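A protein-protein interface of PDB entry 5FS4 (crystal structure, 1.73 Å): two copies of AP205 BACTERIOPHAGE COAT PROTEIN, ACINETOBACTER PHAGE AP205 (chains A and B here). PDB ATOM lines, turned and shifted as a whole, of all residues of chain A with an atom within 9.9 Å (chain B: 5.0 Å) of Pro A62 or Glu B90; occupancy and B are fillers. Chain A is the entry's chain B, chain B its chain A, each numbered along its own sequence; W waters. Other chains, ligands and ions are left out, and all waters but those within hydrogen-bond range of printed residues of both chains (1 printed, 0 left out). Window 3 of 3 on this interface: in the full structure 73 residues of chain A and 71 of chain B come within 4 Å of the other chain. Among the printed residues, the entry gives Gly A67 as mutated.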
ATOM      1  N   ARG A  59     -12.195 -17.709 -11.199  1.00  0.00           N
ATOM      2  CA  ARG A  59     -11.465 -16.671 -11.878  1.00  0.00           C
ATOM      3  C   ARG A  59      -9.970 -16.760 -11.623  1.00  0.00           C
ATOM      4  O   ARG A  59      -9.542 -16.674 -10.483  1.00  0.00           O
ATOM      5  CB  ARG A  59     -11.989 -15.326 -11.358  1.00  0.00           C
ATOM      6  CG  ARG A  59     -11.429 -14.052 -12.024  1.00  0.00           C
ATOM      7  CD  ARG A  59     -11.923 -13.802 -13.431  1.00  0.00           C
ATOM      8  NE  ARG A  59     -13.355 -13.683 -13.488  1.00  0.00           N
ATOM      9  CZ  ARG A  59     -14.066 -13.671 -14.601  1.00  0.00           C
ATOM     10  NH1 ARG A  59     -13.473 -13.731 -15.768  1.00  0.00           N
ATOM     11  NH2 ARG A  59     -15.387 -13.608 -14.523  1.00  0.00           N
ATOM     12  N   PRO A  60      -9.154 -16.893 -12.699  1.00  0.00           N
ATOM     13  CA  PRO A  60      -7.701 -16.890 -12.572  1.00  0.00           C
ATOM     14  C   PRO A  60      -7.213 -15.693 -11.754  1.00  0.00           C
ATOM     15  O   PRO A  60      -7.636 -14.562 -11.980  1.00  0.00           O
ATOM     16  CB  PRO A  60      -7.210 -16.801 -14.047  1.00  0.00           C
ATOM     17  CG  PRO A  60      -8.344 -17.274 -14.860  1.00  0.00           C
ATOM     18  CD  PRO A  60      -9.563 -16.809 -14.121  1.00  0.00           C
ATOM     19  N   ALA A  61      -6.354 -15.965 -10.788  1.00  0.00           N
ATOM     20  CA  ALA A  61      -5.660 -14.888 -10.138  1.00  0.00           C
ATOM     21  C   ALA A  61      -4.823 -14.149 -11.188  1.00  0.00           C
ATOM     22  O   ALA A  61      -4.414 -14.777 -12.172  1.00  0.00           O
ATOM     23  CB  ALA A  61      -4.765 -15.438  -9.026  1.00  0.00           C
ATOM     24  N   PRO A  62      -4.521 -12.838 -10.986  1.00  0.00           N
ATOM     25  CA  PRO A  62      -3.675 -12.116 -11.940  1.00  0.00           C
ATOM     26  C   PRO A  62      -2.254 -12.691 -12.018  1.00  0.00           C
ATOM     27  O   PRO A  62      -1.760 -13.165 -11.016  1.00  0.00           O
ATOM     28  CB  PRO A  62      -3.658 -10.679 -11.364  1.00  0.00           C
ATOM     29  CG  PRO A  62      -4.881 -10.598 -10.519  1.00  0.00           C
ATOM     30  CD  PRO A  62      -5.031 -11.946  -9.930  1.00  0.00           C
ATOM     31  N   LYS A  63      -1.657 -12.712 -13.208  1.00  0.00           N
ATOM     32  CA  LYS A  63      -0.285 -13.233 -13.410  1.00  0.00           C
ATOM     33  C   LYS A  63       0.681 -12.246 -12.850  1.00  0.00           C
ATOM     34  O   LYS A  63       0.461 -11.042 -12.973  1.00  0.00           O
ATOM     35  CB  LYS A  63       0.049 -13.357 -14.899  1.00  0.00           C
ATOM     36  CG  LYS A  63      -0.786 -14.364 -15.640  1.00  0.00           C
ATOM     37  CD  LYS A  63      -0.507 -14.389 -17.131  1.00  0.00           C
ATOM     38  CE  LYS A  63      -1.824 -14.370 -17.896  1.00  0.00           C
ATOM     39  NZ  LYS A  63      -1.697 -14.863 -19.284  1.00  0.00           N
ATOM     40  N   PRO A  64       1.786 -12.714 -12.270  1.00  0.00           N
ATOM     41  CA  PRO A  64       2.764 -11.684 -11.859  1.00  0.00           C
ATOM     42  C   PRO A  64       3.465 -11.016 -13.073  1.00  0.00           C
ATOM     43  O   PRO A  64       3.226 -11.364 -14.274  1.00  0.00           O
ATOM     44  CB  PRO A  64       3.753 -12.469 -10.962  1.00  0.00           C
ATOM     45  CG  PRO A  64       3.687 -13.846 -11.468  1.00  0.00           C
ATOM     46  CD  PRO A  64       2.335 -14.069 -12.126  1.00  0.00           C
ATOM     47  N   GLU A  65       4.310 -10.044 -12.740  1.00  0.00           N
ATOM     48  CA  GLU A  65       5.139  -9.384 -13.720  1.00  0.00           C
ATOM     49  C   GLU A  65       6.002 -10.438 -14.435  1.00  0.00           C
ATOM     50  O   GLU A  65       6.667 -11.261 -13.781  1.00  0.00           O
ATOM     51  CB  GLU A  65       6.019  -8.335 -13.038  1.00  0.00           C
ATOM     52  CG  GLU A  65       5.227  -7.246 -12.334  1.00  0.00           C
ATOM     53  CD  GLU A  65       6.108  -6.149 -11.764  1.00  0.00           C
ATOM     54  OE1 GLU A  65       7.377  -6.216 -11.919  1.00  0.00           O
ATOM     55  OE2 GLU A  65       5.496  -5.219 -11.166  1.00  0.00           O
ATOM     56  N   GLY A  66       5.912 -10.469 -15.761  1.00  0.00           N
ATOM     57  CA  GLY A  66       6.738 -11.360 -16.567  1.00  0.00           C
ATOM     58  C   GLY A  66       6.127 -12.745 -16.733  1.00  0.00           C
ATOM     59  O   GLY A  66       6.737 -13.662 -17.356  1.00  0.00           O
ATOM     60  N   GLY A  67       4.914 -12.904 -16.190  1.00  0.00           N
ATOM     61  CA  GLY A  67       4.194 -14.164 -16.243  1.00  0.00           C
ATOM     62  C   GLY A  67       3.697 -14.589 -17.608  1.00  0.00           C
ATOM     63  O   GLY A  67       3.804 -15.786 -17.934  1.00  0.00           O
ATOM     64  N   ALA A  68       3.175 -13.649 -18.410  1.00  0.00           N
ATOM     65  CA  ALA A  68       2.707 -13.964 -19.797  1.00  0.00           C
ATOM     66  C   ALA A  68       3.849 -14.537 -20.656  1.00  0.00           C
ATOM     67  O   ALA A  68       3.751 -15.632 -21.253  1.00  0.00           O
ATOM     68  CB  ALA A  68       2.135 -12.724 -20.461  1.00  0.00           C
ATOM     69  N   VAL A  72       2.866 -18.553 -17.780  1.00  0.00           N
ATOM     70  CA  VAL A  72       2.235 -18.910 -16.500  1.00  0.00           C
ATOM     71  C   VAL A  72       0.718 -19.051 -16.699  1.00  0.00           C
ATOM     72  O   VAL A  72       0.091 -18.202 -17.376  1.00  0.00           O
ATOM     73  CB  VAL A  72       2.532 -17.864 -15.404  1.00  0.00           C
ATOM     74  CG1 VAL A  72       1.731 -18.136 -14.113  1.00  0.00           C
ATOM     75  CG2 VAL A  72       4.017 -17.855 -15.107  1.00  0.00           C
ATOM     76  N   ILE A  73       0.156 -20.131 -16.145  1.00  0.00           N
ATOM     77  CA  ILE A  73      -1.285 -20.259 -15.946  1.00  0.00           C
ATOM     78  C   ILE A  73      -1.508 -20.229 -14.456  1.00  0.00           C
ATOM     79  O   ILE A  73      -1.042 -21.128 -13.733  1.00  0.00           O
ATOM     80  CB  ILE A  73      -1.875 -21.580 -16.457  1.00  0.00           C
ATOM     81  CG1 ILE A  73      -1.462 -21.864 -17.916  1.00  0.00           C
ATOM     82  CG2 ILE A  73      -3.387 -21.567 -16.303  1.00  0.00           C
ATOM     83  CD1 ILE A  73      -1.648 -20.737 -18.869  1.00  0.00           C
ATOM     84  N   MET A  74      -2.268 -19.222 -13.993  1.00  0.00           N
ATOM     85  CA  MET A  74      -2.500 -19.049 -12.536  1.00  0.00           C
ATOM     86  C   MET A  74      -3.681 -19.914 -11.998  1.00  0.00           C
ATOM     87  O   MET A  74      -4.546 -20.297 -12.760  1.00  0.00           O
ATOM     88  CB  MET A  74      -2.703 -17.536 -12.220  1.00  0.00           C
ATOM     89  CG  MET A  74      -1.441 -16.684 -12.503  1.00  0.00           C
ATOM     90  SD  MET A  74      -0.126 -16.991 -11.326  1.00  0.00           S
ATOM     91  CE  MET A  74      -0.743 -16.155  -9.889  1.00  0.00           C
ATOM     92  N   PRO A  75      -3.664 -20.273 -10.714  1.00  0.00           N
ATOM     93  CA  PRO A  75      -4.814 -20.979 -10.134  1.00  0.00           C
ATOM     94  C   PRO A  75      -6.042 -20.067 -10.065  1.00  0.00           C
ATOM     95  O   PRO A  75      -5.871 -18.830 -10.157  1.00  0.00           O
ATOM     96  CB  PRO A  75      -4.352 -21.319  -8.722  1.00  0.00           C
ATOM     97  CG  PRO A  75      -3.291 -20.305  -8.431  1.00  0.00           C
ATOM     98  CD  PRO A  75      -2.604 -20.021  -9.727  1.00  0.00           C
ATOM     99  N   ASN A  76      -7.225 -20.645  -9.836  1.00  0.00           N
ATOM    100  CA  ASN A  76      -8.455 -19.823  -9.739  1.00  0.00           C
ATOM    101  C   ASN A  76      -8.875 -19.550  -8.323  1.00  0.00           C
ATOM    102  O   ASN A  76      -8.770 -20.388  -7.445  1.00  0.00           O
ATOM    103  CB  ASN A  76      -9.636 -20.467 -10.453  1.00  0.00           C
ATOM    104  CG  ASN A  76      -9.355 -20.742 -11.917  1.00  0.00           C
ATOM    105  OD1 ASN A  76      -8.791 -19.933 -12.607  1.00  0.00           O
ATOM    106  ND2 ASN A  76      -9.808 -21.870 -12.395  1.00  0.00           N
ATOM    107  N   GLU A  77      -9.419 -18.362  -8.161  1.00  0.00           N
ATOM    108  CA  GLU A  77     -10.194 -17.974  -7.003  1.00  0.00           C
ATOM    109  C   GLU A  77     -11.628 -18.247  -7.248  1.00  0.00           C
ATOM    110  O   GLU A  77     -12.039 -18.502  -8.356  1.00  0.00           O
ATOM    111  CB  GLU A  77      -9.997 -16.466  -6.683  1.00  0.00           C
ATOM    112  CG  GLU A  77     -10.573 -15.449  -7.678  1.00  0.00           C
ATOM    113  CD  GLU A  77     -10.780 -14.075  -7.046  1.00  0.00           C
ATOM    114  OE1 GLU A  77     -11.095 -14.004  -5.835  1.00  0.00           O
ATOM    115  OE2 GLU A  77     -10.642 -13.045  -7.779  1.00  0.00           O
ATOM    116  N   GLN A  79     -15.098 -16.415  -7.144  1.00  0.00           N
ATOM    117  CA  GLN A  79     -15.896 -15.203  -7.108  1.00  0.00           C
ATOM    118  C   GLN A  79     -17.325 -15.635  -6.854  1.00  0.00           C
ATOM    119  O   GLN A  79     -17.925 -16.265  -7.722  1.00  0.00           O
ATOM    120  CB  GLN A  79     -15.809 -14.465  -8.461  1.00  0.00           C
ATOM    121  CG  GLN A  79     -14.448 -13.789  -8.696  1.00  0.00           C
ATOM    122  CD  GLN A  79     -14.379 -13.008  -9.977  1.00  0.00           C
ATOM    123  OE1 GLN A  79     -14.881 -13.462 -11.031  1.00  0.00           O
ATOM    124  NE2 GLN A  79     -13.698 -11.849  -9.931  1.00  0.00           N
ATOM    125  N   GLY A 116     -15.768  -2.711  -3.030  1.00  0.00           N
ATOM    126  CA  GLY A 116     -15.070  -3.893  -3.490  1.00  0.00           C
ATOM    127  C   GLY A 116     -13.578  -3.956  -3.169  1.00  0.00           C
ATOM    128  O   GLY A 116     -12.991  -5.051  -3.149  1.00  0.00           O
ATOM    129  N   LEU A 117     -12.986  -2.786  -2.882  1.00  0.00           N
ATOM    130  CA  LEU A 117     -11.611  -2.707  -2.322  1.00  0.00           C
ATOM    131  C   LEU A 117     -11.581  -2.874  -0.783  1.00  0.00           C
ATOM    132  O   LEU A 117     -10.499  -2.929  -0.161  1.00  0.00           O
ATOM    133  CB  LEU A 117     -11.001  -1.349  -2.736  1.00  0.00           C
ATOM    134  CG  LEU A 117     -10.844  -1.112  -4.241  1.00  0.00           C
ATOM    135  CD1 LEU A 117     -10.079   0.176  -4.501  1.00  0.00           C
ATOM    136  CD2 LEU A 117     -10.169  -2.273  -4.974  1.00  0.00           C
ATOM    137  N   GLY A 118     -12.753  -2.950  -0.169  1.00  0.00           N
ATOM    138  CA  GLY A 118     -12.873  -3.113   1.292  1.00  0.00           C
ATOM    139  C   GLY A 118     -13.088  -1.849   2.119  1.00  0.00           C
ATOM    140  O   GLY A 118     -12.954  -1.905   3.323  1.00  0.00           O
ATOM    141  N   GLU B  45      -1.710 -15.518  -3.484  1.00  0.00           N
ATOM    142  CA  GLU B  45      -1.722 -14.459  -2.442  1.00  0.00           C
ATOM    143  C   GLU B  45      -2.620 -13.196  -2.624  1.00  0.00           C
ATOM    144  O   GLU B  45      -2.102 -12.143  -2.895  1.00  0.00           O
ATOM    145  CB  GLU B  45      -0.282 -13.958  -2.231  1.00  0.00           C
ATOM    146  N   LEU B  46      -3.933 -13.290  -2.371  1.00  0.00           N
ATOM    147  CA  LEU B  46      -4.924 -12.231  -2.725  1.00  0.00           C
ATOM    148  C   LEU B  46      -5.552 -11.619  -1.488  1.00  0.00           C
ATOM    149  O   LEU B  46      -5.399 -12.151  -0.406  1.00  0.00           O
ATOM    150  CB  LEU B  46      -6.036 -12.859  -3.580  1.00  0.00           C
ATOM    151  CG  LEU B  46      -5.577 -13.520  -4.915  1.00  0.00           C
ATOM    152  CD1 LEU B  46      -6.716 -14.182  -5.660  1.00  0.00           C
ATOM    153  CD2 LEU B  46      -4.883 -12.564  -5.874  1.00  0.00           C
ATOM    154  N   ASN B  47      -6.288 -10.520  -1.644  1.00  0.00           N
ATOM    155  CA  ASN B  47      -7.064  -9.964  -0.562  1.00  0.00           C
ATOM    156  C   ASN B  47      -8.541 -10.077  -0.880  1.00  0.00           C
ATOM    157  O   ASN B  47      -9.089  -9.257  -1.649  1.00  0.00           O
ATOM    158  CB  ASN B  47      -6.678  -8.525  -0.358  1.00  0.00           C
ATOM    159  CG  ASN B  47      -5.210  -8.367  -0.024  1.00  0.00           C
ATOM    160  OD1 ASN B  47      -4.832  -8.424   1.130  1.00  0.00           O
ATOM    161  ND2 ASN B  47      -4.382  -8.177  -1.048  1.00  0.00           N
ATOM    162  N   SER B  88     -11.613 -11.450  -4.498  1.00  0.00           N
ATOM    163  CA  SER B  88     -10.423 -10.637  -4.324  1.00  0.00           C
ATOM    164  C   SER B  88     -10.575  -9.219  -4.882  1.00  0.00           C
ATOM    165  O   SER B  88     -11.191  -8.994  -5.943  1.00  0.00           O
ATOM    166  CB  SER B  88      -9.245 -11.284  -5.023  1.00  0.00           C
ATOM    167  OG  SER B  88      -9.351 -11.102  -6.406  1.00  0.00           O
ATOM    168  N   ALA B  89      -9.999  -8.253  -4.162  1.00  0.00           N
ATOM    169  CA  ALA B  89      -9.864  -6.913  -4.687  1.00  0.00           C
ATOM    170  C   ALA B  89      -9.100  -6.900  -6.017  1.00  0.00           C
ATOM    171  O   ALA B  89      -9.382  -6.101  -6.925  1.00  0.00           O
ATOM    172  CB  ALA B  89      -9.185  -6.018  -3.644  1.00  0.00           C
ATOM    173  N   GLU B  90      -8.106  -7.770  -6.128  1.00  0.00           N
ATOM    174  CA  GLU B  90      -7.239  -7.803  -7.333  1.00  0.00           C
ATOM    175  C   GLU B  90      -8.049  -8.023  -8.600  1.00  0.00           C
ATOM    176  O   GLU B  90      -7.775  -7.426  -9.632  1.00  0.00           O
ATOM    177  CB  GLU B  90      -6.105  -8.863  -7.147  1.00  0.00           C
ATOM    178  CG  GLU B  90      -5.057  -8.510  -6.096  1.00  0.00           C
ATOM    179  CD  GLU B  90      -5.440  -8.744  -4.619  1.00  0.00           C
ATOM    180  OE1 GLU B  90      -6.575  -9.231  -4.234  1.00  0.00           O
ATOM    181  OE2 GLU B  90      -4.582  -8.372  -3.758  1.00  0.00           O
ATOM    182  N   ASN B  91      -9.124  -8.832  -8.500  1.00  0.00           N
ATOM    183  CA  ASN B  91      -9.988  -9.128  -9.661  1.00  0.00           C
ATOM    184  C   ASN B  91     -11.304  -8.414  -9.602  1.00  0.00           C
ATOM    185  O   ASN B  91     -12.304  -8.872 -10.192  1.00  0.00           O
ATOM    186  CB  ASN B  91     -10.226 -10.639  -9.783  1.00  0.00           C
ATOM    187  CG  ASN B  91      -9.073 -11.366 -10.478  1.00  0.00           C
ATOM    188  OD1 ASN B  91      -8.476 -10.836 -11.388  1.00  0.00           O
ATOM    189  ND2 ASN B  91      -8.822 -12.610 -10.097  1.00  0.00           N
ATOM    190  N   LEU B  92     -11.299  -7.270  -8.931  1.00  0.00           N
ATOM    191  CA  LEU B  92     -12.504  -6.466  -8.804  1.00  0.00           C
ATOM    192  C   LEU B  92     -13.196  -6.071 -10.142  1.00  0.00           C
ATOM    193  O   LEU B  92     -14.422  -5.998 -10.213  1.00  0.00           O
ATOM    194  CB  LEU B  92     -12.191  -5.218  -7.986  1.00  0.00           C
ATOM    195  CG  LEU B  92     -13.398  -4.283  -7.826  1.00  0.00           C
ATOM    196  CD1 LEU B  92     -14.468  -5.056  -7.037  1.00  0.00           C
ATOM    197  CD2 LEU B  92     -12.995  -3.021  -7.119  1.00  0.00           C
HETATM  198  O   HOH W   1     -12.550 -11.066  -7.379  1.00  0.00           O
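The side-chain hydroxyl of Ser B88 lies within hydrogen-bond range of the side-chain carboxylate of Glu A77, at 2.7 Å.
The side-chain amide nitrogen (ND2) of Asn B91 sits at hydrogen-bond distance from the backbone carbonyl oxygen (O) of Pro A60.
ND2 of Asn B91 is in hydrogen-bond range of OE2 of Glu A77, 3.0 Å away.
O of Asn B91 is in hydrogen-bond range of NE2 of Gln A79 (3.3 Å).
O of Asn B47 lies within hydrogen-bond range of N of Ala B89, 2.9 Å away.
The side-chain amide nitrogen (ND2) of Asn B47 is in hydrogen-bond range of the side-chain carboxylate (OE2) of Glu B90.
The backbone NH (N) of Asn B91 sits at hydrogen-bond distance from the side-chain hydroxyl (OG) of Ser B88, 3.1 Å away.
O of Arg A59 lies within hydrogen-bond range of N of Glu A77 (2.9 Å).
The guanidinium group of Arg A59 is in hydrogen-bond range of the side-chain amide oxygen of Gln A79 (2.9 Å).
The backbone carbonyl oxygen of Pro A75 lies within hydrogen-bond range of the backbone NH of Ala A61.
Among the printed residues, pairs that only touch across the chains: Arg A59 with Asn B91, Leu A117 with Leu B92, Pro A62 with Asn B91, Gly A116 with Leu B92, Ala A61 with Asn B91, Gly A116 with Ala B89 and Pro A62 with Glu B90.
Printed residues of chain B within 4 Å of Arg A59: Asn B91 (3.5 Å).
Printed residues of chain B within 4 Å of Pro A60: Asn B91.
Printed residues of chain B within 4 Å of Ala A61: Asn B91.
Printed residues of chain B within 4 Å of Pro A62: Glu B90 (3.98 Å) and Asn B91 (3.7 Å).
Printed residues of chain B within 4 Å of Gly A116: Ala B89 (3.95 Å) and Leu B92 (3.8 Å).
Printed residues of chain B within 4 Å of Leu A117: Leu B92 (3.6 Å).
Leu B46 touches none of the printed residues of chain A.
Asn B47 touches none of the printed residues of chain A.
Of the printed residues of chain A, Glu B90 touches Pro A62.
Printed residues of chain A within 4 Å of Asn B91: Arg A59, Pro A60, Ala A61, Pro A62, Glu A77 and Gln A79.
The nearest printed residue of chain B that does not touch Pro A62 is Leu B46 (4.1 Å).
Of the 8 printed residues of chain B, 5 touch a printed residue of chain A.
Printed residues of chain B that touch a printed residue of chain A: Ser B88, Ala B89, Glu B90, Asn B91 and Leu B92.
Hydrophobic or aromatic side chains of chain B within 4 Å of the printed part of chain A: Ala B89 and Leu B92.
Among the printed residues, 11 pairs touch across the chains.
Among the printed residues, no Asp or Glu carboxylate lies within 4 Å of a Lys or Arg side-chain nitrogen of the other chain.
No position is printed for both chains.
Of the 11 pairs that touch across the chains among the printed residues, none has its exchanged pair printed and touching as well.
Water W1 lies within hydrogen-bond range of OE2 of Glu A77 (2.8 Å), O of Ser B88 (2.9 Å) and NE2 of Gln A79 (2.9 Å).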
